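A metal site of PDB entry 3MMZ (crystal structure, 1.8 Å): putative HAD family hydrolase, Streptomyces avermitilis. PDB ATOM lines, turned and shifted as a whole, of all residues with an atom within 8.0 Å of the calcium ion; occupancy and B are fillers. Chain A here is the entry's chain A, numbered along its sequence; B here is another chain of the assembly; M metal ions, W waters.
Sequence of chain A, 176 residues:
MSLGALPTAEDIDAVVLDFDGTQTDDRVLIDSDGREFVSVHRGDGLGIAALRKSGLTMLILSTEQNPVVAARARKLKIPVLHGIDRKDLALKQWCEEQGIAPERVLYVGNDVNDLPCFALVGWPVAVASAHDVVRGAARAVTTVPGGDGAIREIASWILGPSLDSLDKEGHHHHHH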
ATOM      1  N   ASP A  18     -19.846  -4.900  31.205  1.00  0.00           N
ATOM      2  CA  ASP A  18     -18.568  -5.486  30.889  1.00  0.00           C
ATOM      3  C   ASP A  18     -17.781  -5.527  32.203  1.00  0.00           C
ATOM      4  O   ASP A  18     -18.140  -4.835  33.151  1.00  0.00           O
ATOM      5  CB  ASP A  18     -17.837  -4.629  29.862  1.00  0.00           C
ATOM      6  CG  ASP A  18     -16.458  -5.174  29.509  1.00  0.00           C
ATOM      7  OD1 ASP A  18     -16.329  -6.393  29.259  1.00  0.00           O
ATOM      8  OD2 ASP A  18     -15.511  -4.371  29.473  1.00  0.00           O
ATOM      9  N   PHE A  19     -16.734  -6.338  32.256  1.00  0.00           N
ATOM     10  CA  PHE A  19     -15.894  -6.404  33.448  1.00  0.00           C
ATOM     11  C   PHE A  19     -14.554  -5.723  33.275  1.00  0.00           C
ATOM     12  O   PHE A  19     -14.389  -4.574  33.694  1.00  0.00           O
ATOM     13  CB  PHE A  19     -15.716  -7.859  33.893  1.00  0.00           C
ATOM     14  CG  PHE A  19     -15.039  -7.993  35.218  1.00  0.00           C
ATOM     15  CD1 PHE A  19     -15.653  -7.516  36.368  1.00  0.00           C
ATOM     16  CD2 PHE A  19     -13.785  -8.580  35.318  1.00  0.00           C
ATOM     17  CE1 PHE A  19     -15.036  -7.624  37.624  1.00  0.00           C
ATOM     18  CE2 PHE A  19     -13.146  -8.709  36.576  1.00  0.00           C
ATOM     19  CZ  PHE A  19     -13.775  -8.232  37.725  1.00  0.00           C
ATOM     20  N   ASP A  20     -13.582  -6.389  32.649  1.00  0.00           N
ATOM     21  CA  ASP A  20     -12.210  -5.811  32.572  1.00  0.00           C
ATOM     22  C   ASP A  20     -12.243  -4.491  31.797  1.00  0.00           C
ATOM     23  O   ASP A  20     -12.813  -4.434  30.687  1.00  0.00           O
ATOM     24  CB  ASP A  20     -11.241  -6.788  31.891  1.00  0.00           C
ATOM     25  CG  ASP A  20     -11.093  -8.085  32.638  1.00  0.00           C
ATOM     26  OD1 ASP A  20     -10.384  -8.118  33.668  1.00  0.00           O
ATOM     27  OD2 ASP A  20     -11.668  -9.098  32.197  1.00  0.00           O
ATOM     28  N   GLY A  21     -11.667  -3.427  32.370  1.00  0.00           N
ATOM     29  CA  GLY A  21     -11.621  -2.135  31.689  1.00  0.00           C
ATOM     30  C   GLY A  21     -12.843  -1.272  31.942  1.00  0.00           C
ATOM     31  O   GLY A  21     -12.835  -0.075  31.628  1.00  0.00           O
ATOM     32  N   THR A  22     -13.869  -1.879  32.519  1.00  0.00           N
ATOM     33  CA  THR A  22     -15.126  -1.197  32.777  1.00  0.00           C
ATOM     34  C   THR A  22     -15.353  -1.104  34.279  1.00  0.00           C
ATOM     35  O   THR A  22     -15.598   0.005  34.803  1.00  0.00           O
ATOM     36  CB  THR A  22     -16.286  -1.908  32.028  1.00  0.00           C
ATOM     37  OG1 THR A  22     -16.104  -1.746  30.607  1.00  0.00           O
ATOM     38  CG2 THR A  22     -17.634  -1.335  32.426  1.00  0.00           C
ATOM     39  N   GLN A  23     -15.249  -2.244  34.962  1.00  0.00           N
ATOM     40  CA  GLN A  23     -15.217  -2.323  36.424  1.00  0.00           C
ATOM     41  C   GLN A  23     -13.781  -2.380  36.977  1.00  0.00           C
ATOM     42  O   GLN A  23     -13.575  -2.435  38.189  1.00  0.00           O
ATOM     43  CB  GLN A  23     -15.997  -3.540  36.909  1.00  0.00           C
ATOM     44  CG  GLN A  23     -17.472  -3.472  36.584  1.00  0.00           C
ATOM     45  CD  GLN A  23     -18.210  -4.716  36.999  1.00  0.00           C
ATOM     46  OE1 GLN A  23     -18.369  -4.969  38.183  1.00  0.00           O
ATOM     47  NE2 GLN A  23     -18.690  -5.483  36.024  1.00  0.00           N
ATOM     48  N   THR A  24     -12.800  -2.408  36.062  1.00  0.00           N
ATOM     49  CA  THR A  24     -11.387  -2.402  36.414  1.00  0.00           C
ATOM     50  C   THR A  24     -10.654  -1.433  35.480  1.00  0.00           C
ATOM     51  O   THR A  24     -11.199  -0.982  34.472  1.00  0.00           O
ATOM     52  CB  THR A  24     -10.717  -3.805  36.254  1.00  0.00           C
ATOM     53  OG1 THR A  24     -10.436  -4.024  34.867  1.00  0.00           O
ATOM     54  CG2 THR A  24     -11.589  -4.949  36.794  1.00  0.00           C
ATOM     55  N   ASP A  26      -8.395  -2.333  33.590  1.00  0.00           N
ATOM     56  CA  ASP A  26      -7.903  -3.198  32.494  1.00  0.00           C
ATOM     57  C   ASP A  26      -6.598  -3.920  32.826  1.00  0.00           C
ATOM     58  O   ASP A  26      -6.082  -4.643  31.988  1.00  0.00           O
ATOM     59  CB  ASP A  26      -7.762  -2.424  31.161  1.00  0.00           C
ATOM     60  CG  ASP A  26      -8.659  -2.974  30.040  1.00  0.00           C
ATOM     61  OD1 ASP A  26      -9.373  -3.993  30.204  1.00  0.00           O
ATOM     62  OD2 ASP A  26      -8.635  -2.380  28.940  1.00  0.00           O
ATOM     63  N   LEU A  61     -21.261  -9.489  31.806  1.00  0.00           N
ATOM     64  CA  LEU A  61     -20.956 -10.287  30.613  1.00  0.00           C
ATOM     65  C   LEU A  61     -19.466 -10.273  30.345  1.00  0.00           C
ATOM     66  O   LEU A  61     -18.856  -9.202  30.295  1.00  0.00           O
ATOM     67  CB  LEU A  61     -21.652  -9.700  29.379  1.00  0.00           C
ATOM     68  CG  LEU A  61     -22.971 -10.213  28.820  1.00  0.00           C
ATOM     69  CD1 LEU A  61     -23.212  -9.566  27.447  1.00  0.00           C
ATOM     70  CD2 LEU A  61     -22.981 -11.731  28.717  1.00  0.00           C
ATOM     71  N   SER A  62     -18.873 -11.449  30.137  1.00  0.00           N
ATOM     72  CA  SER A  62     -17.470 -11.531  29.761  1.00  0.00           C
ATOM     73  C   SER A  62     -17.240 -12.712  28.830  1.00  0.00           C
ATOM     74  O   SER A  62     -17.735 -13.806  29.066  1.00  0.00           O
ATOM     75  CB  SER A  62     -16.589 -11.659  31.011  1.00  0.00           C
ATOM     76  OG  SER A  62     -15.268 -12.076  30.688  1.00  0.00           O
ATOM     77  N   LYS A  87     -20.509 -12.335  22.994  1.00  0.00           N
ATOM     78  CA  LYS A  87     -21.184 -11.515  24.007  1.00  0.00           C
ATOM     79  C   LYS A  87     -22.559 -11.062  23.536  1.00  0.00           C
ATOM     80  O   LYS A  87     -23.524 -11.132  24.308  1.00  0.00           O
ATOM     81  CB  LYS A  87     -20.356 -10.263  24.334  1.00  0.00           C
ATOM     82  CG  LYS A  87     -19.228 -10.486  25.302  1.00  0.00           C
ATOM     83  CD  LYS A  87     -18.204  -9.375  25.200  1.00  0.00           C
ATOM     84  CE  LYS A  87     -18.437  -8.282  26.211  1.00  0.00           C
ATOM     85  NZ  LYS A  87     -17.160  -7.526  26.430  1.00  0.00           N
ATOM     86  N   TYR A 107     -25.972  -0.872  28.557  1.00  0.00           N
ATOM     87  CA  TYR A 107     -24.777  -1.717  28.545  1.00  0.00           C
ATOM     88  C   TYR A 107     -23.538  -0.839  28.637  1.00  0.00           C
ATOM     89  O   TYR A 107     -23.399   0.101  27.872  1.00  0.00           O
ATOM     90  CB  TYR A 107     -24.746  -2.557  27.251  1.00  0.00           C
ATOM     91  CG  TYR A 107     -23.503  -3.407  27.170  1.00  0.00           C
ATOM     92  CD1 TYR A 107     -23.486  -4.699  27.683  1.00  0.00           C
ATOM     93  CD2 TYR A 107     -22.331  -2.903  26.601  1.00  0.00           C
ATOM     94  CE1 TYR A 107     -22.317  -5.500  27.621  1.00  0.00           C
ATOM     95  CE2 TYR A 107     -21.169  -3.669  26.518  1.00  0.00           C
ATOM     96  CZ  TYR A 107     -21.174  -4.959  27.035  1.00  0.00           C
ATOM     97  OH  TYR A 107     -20.021  -5.709  26.968  1.00  0.00           O
ATOM     98  N   VAL A 108     -22.630  -1.176  29.567  1.00  0.00           N
ATOM     99  CA  VAL A 108     -21.397  -0.384  29.798  1.00  0.00           C
ATOM    100  C   VAL A 108     -20.189  -1.151  29.294  1.00  0.00           C
ATOM    101  O   VAL A 108     -20.027  -2.331  29.617  1.00  0.00           O
ATOM    102  CB  VAL A 108     -21.188  -0.040  31.297  1.00  0.00           C
ATOM    103  CG1 VAL A 108     -20.125   1.047  31.437  1.00  0.00           C
ATOM    104  CG2 VAL A 108     -22.507   0.424  31.938  1.00  0.00           C
ATOM    105  N   GLY A 109     -19.354  -0.480  28.499  1.00  0.00           N
ATOM    106  CA  GLY A 109     -18.178  -1.135  27.896  1.00  0.00           C
ATOM    107  C   GLY A 109     -17.020  -0.175  27.706  1.00  0.00           C
ATOM    108  O   GLY A 109     -17.146   1.016  28.020  1.00  0.00           O
ATOM    109  N   ASN A 110     -15.895  -0.699  27.222  1.00  0.00           N
ATOM    110  CA  ASN A 110     -14.669   0.099  27.078  1.00  0.00           C
ATOM    111  C   ASN A 110     -13.871  -0.162  25.816  1.00  0.00           C
ATOM    112  O   ASN A 110     -12.994   0.637  25.493  1.00  0.00           O
ATOM    113  CB  ASN A 110     -13.731  -0.120  28.284  1.00  0.00           C
ATOM    114  CG  ASN A 110     -13.007  -1.445  28.214  1.00  0.00           C
ATOM    115  OD1 ASN A 110     -13.638  -2.511  28.252  1.00  0.00           O
ATOM    116  ND2 ASN A 110     -11.675  -1.403  28.134  1.00  0.00           N
ATOM    117  N   ASP A 111     -14.088  -1.279  25.121  1.00  0.00           N
ATOM    118  CA  ASP A 111     -13.217  -1.620  23.981  1.00  0.00           C
ATOM    119  C   ASP A 111     -14.011  -2.196  22.820  1.00  0.00           C
ATOM    120  O   ASP A 111     -15.251  -2.361  22.880  1.00  0.00           O
ATOM    121  CB  ASP A 111     -12.045  -2.545  24.401  1.00  0.00           C
ATOM    122  CG  ASP A 111     -10.736  -2.286  23.581  1.00  0.00           C
ATOM    123  OD1 ASP A 111     -10.765  -1.727  22.444  1.00  0.00           O
ATOM    124  OD2 ASP A 111      -9.653  -2.650  24.097  1.00  0.00           O
ATOM    125  N   VAL A 112     -13.310  -2.469  21.721  1.00  0.00           N
ATOM    126  CA  VAL A 112     -13.986  -2.768  20.441  1.00  0.00           C
ATOM    127  C   VAL A 112     -14.803  -4.059  20.456  1.00  0.00           C
ATOM    128  O   VAL A 112     -15.743  -4.225  19.671  1.00  0.00           O
ATOM    129  CB  VAL A 112     -13.008  -2.721  19.246  1.00  0.00           C
ATOM    130  CG1 VAL A 112     -12.501  -1.299  19.052  1.00  0.00           C
ATOM    131  CG2 VAL A 112     -11.853  -3.666  19.451  1.00  0.00           C
ATOM    132  N   ASN A 113     -14.451  -4.958  21.367  1.00  0.00           N
ATOM    133  CA  ASN A 113     -15.243  -6.191  21.560  1.00  0.00           C
ATOM    134  C   ASN A 113     -16.610  -5.932  22.198  1.00  0.00           C
ATOM    135  O   ASN A 113     -17.423  -6.862  22.318  1.00  0.00           O
ATOM    136  CB  ASN A 113     -14.433  -7.254  22.333  1.00  0.00           C
ATOM    137  CG  ASN A 113     -13.885  -6.742  23.671  1.00  0.00           C
ATOM    138  OD1 ASN A 113     -13.684  -5.543  23.884  1.00  0.00           O
ATOM    139  ND2 ASN A 113     -13.637  -7.676  24.577  1.00  0.00           N
ATOM    140  N   ASP A 114     -16.880  -4.691  22.593  1.00  0.00           N
ATOM    141  CA  ASP A 114     -18.198  -4.307  23.082  1.00  0.00           C
ATOM    142  C   ASP A 114     -19.098  -3.726  22.006  1.00  0.00           C
ATOM    143  O   ASP A 114     -20.293  -3.495  22.261  1.00  0.00           O
ATOM    144  CB  ASP A 114     -18.068  -3.299  24.221  1.00  0.00           C
ATOM    145  CG  ASP A 114     -17.369  -3.877  25.421  1.00  0.00           C
ATOM    146  OD1 ASP A 114     -17.829  -4.940  25.907  1.00  0.00           O
ATOM    147  OD2 ASP A 114     -16.365  -3.285  25.866  1.00  0.00           O
ATOM    148  N   VAL A 127     -17.134   3.947  29.314  1.00  0.00           N
ATOM    149  CA  VAL A 127     -16.401   4.555  30.420  1.00  0.00           C
ATOM    150  C   VAL A 127     -15.443   5.595  29.830  1.00  0.00           C
ATOM    151  O   VAL A 127     -15.120   5.527  28.640  1.00  0.00           O
ATOM    152  CB  VAL A 127     -15.665   3.513  31.307  1.00  0.00           C
ATOM    153  CG1 VAL A 127     -16.679   2.596  31.997  1.00  0.00           C
ATOM    154  CG2 VAL A 127     -14.608   2.710  30.491  1.00  0.00           C
ATOM    155  N   HIS A 131     -11.681   3.301  24.459  1.00  0.00           N
ATOM    156  CA  HIS A 131     -10.983   3.632  23.234  1.00  0.00           C
ATOM    157  C   HIS A 131     -11.846   4.505  22.331  1.00  0.00           C
ATOM    158  O   HIS A 131     -13.061   4.481  22.454  1.00  0.00           O
ATOM    159  CB  HIS A 131     -10.525   2.345  22.547  1.00  0.00           C
ATOM    160  CG  HIS A 131      -9.476   1.633  23.330  1.00  0.00           C
ATOM    161  ND1 HIS A 131      -8.129   1.855  23.136  1.00  0.00           N
ATOM    162  CD2 HIS A 131      -9.577   0.780  24.377  1.00  0.00           C
ATOM    163  CE1 HIS A 131      -7.440   1.134  23.995  1.00  0.00           C
ATOM    164  NE2 HIS A 131      -8.294   0.465  24.764  1.00  0.00           N
ATOM    165  N   ARG B  42      -5.200  -5.991  29.707  1.00  0.00           N
ATOM    166  CA  ARG B  42      -6.200  -6.744  28.928  1.00  0.00           C
ATOM    167  C   ARG B  42      -6.379  -6.161  27.525  1.00  0.00           C
ATOM    168  O   ARG B  42      -6.715  -6.882  26.583  1.00  0.00           O
ATOM    169  CB  ARG B  42      -7.540  -6.781  29.660  1.00  0.00           C
ATOM    170  CG  ARG B  42      -7.566  -7.715  30.882  1.00  0.00           C
ATOM    171  CD  ARG B  42      -8.169  -9.055  30.541  1.00  0.00           C
ATOM    172  NE  ARG B  42      -8.451  -9.873  31.710  1.00  0.00           N
ATOM    173  CZ  ARG B  42      -7.756 -10.960  32.064  1.00  0.00           C
ATOM    174  NH1 ARG B  42      -6.717 -11.362  31.343  1.00  0.00           N
ATOM    175  NH2 ARG B  42      -8.116 -11.640  33.150  1.00  0.00           N
ATOM    176  N   GLY B  43      -6.200  -4.845  27.402  1.00  0.00           N
ATOM    177  CA  GLY B  43      -6.207  -4.168  26.100  1.00  0.00           C
ATOM    178  C   GLY B  43      -5.066  -4.707  25.243  1.00  0.00           C
ATOM    179  O   GLY B  43      -5.267  -5.029  24.078  1.00  0.00           O
ATOM    180  N   LEU B  46      -6.086  -8.051  23.997  1.00  0.00           N
ATOM    181  CA  LEU B  46      -7.018  -7.946  22.857  1.00  0.00           C
ATOM    182  C   LEU B  46      -6.276  -7.645  21.550  1.00  0.00           C
ATOM    183  O   LEU B  46      -6.565  -8.249  20.492  1.00  0.00           O
ATOM    184  CB  LEU B  46      -8.066  -6.867  23.135  1.00  0.00           C
ATOM    185  CG  LEU B  46      -9.290  -6.817  22.225  1.00  0.00           C
ATOM    186  CD1 LEU B  46     -10.077  -8.121  22.316  1.00  0.00           C
ATOM    187  CD2 LEU B  46     -10.160  -5.645  22.628  1.00  0.00           C
HETATM  188 CA    CA M   1     -13.451  -4.815  28.522  1.00  0.00          CA
HETATM  189  O   HOH W   1     -14.739  -5.265  26.620  1.00  0.00           O
HETATM  190  O   HOH W   2     -13.524  -7.296  28.760  1.00  0.00           O
HETATM  191  O   HOH W   3     -11.146  -4.616  28.344  1.00  0.00           O
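OD1 of Asp 20 lies within salt-bridge range of NE of Arg 42 of chain B (3.3 Å). OD2 of Asp 18 lies close to OG1 of Thr 22. The side-chain carboxylate of Asp 18 lies within salt-bridge range of the side-chain amino group of Lys 87, at 3.2 Å. O of Val 108 lies within hydrogen-bond range of N of Asp 18, 3.0 Å away. The backbone carbonyl oxygen of Asp 18 is in hydrogen-bond range of the side-chain amide nitrogen of Gln 23, at 3.0 Å. N of Asn 110 lies within hydrogen-bond range of OD2 of Asp 114 (3.0 Å). ND2 of Asn 110 lies within hydrogen-bond range of OD2 of Asp 26. O of Asn 110 sits at hydrogen-bond distance from N of His 131.
The nearest printed residue that does not touch the calcium ion is Asp 114 (4.2 Å).
The calcium ion is bound by the backbone carbonyl oxygen of Asp 20 (2.3 Å), the side-chain carboxylate of Asp 18 (2.3 Å), water W3 (2.3 Å), the side-chain amide oxygen of Asn 110 (2.3 Å), water W1 (2.3 Å) and water W2 (2.5 Å).
Water W3 bridges the side-chain carboxylate (OD1) of Asp 26 and the side-chain amide nitrogen (ND2) of Asn 110.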
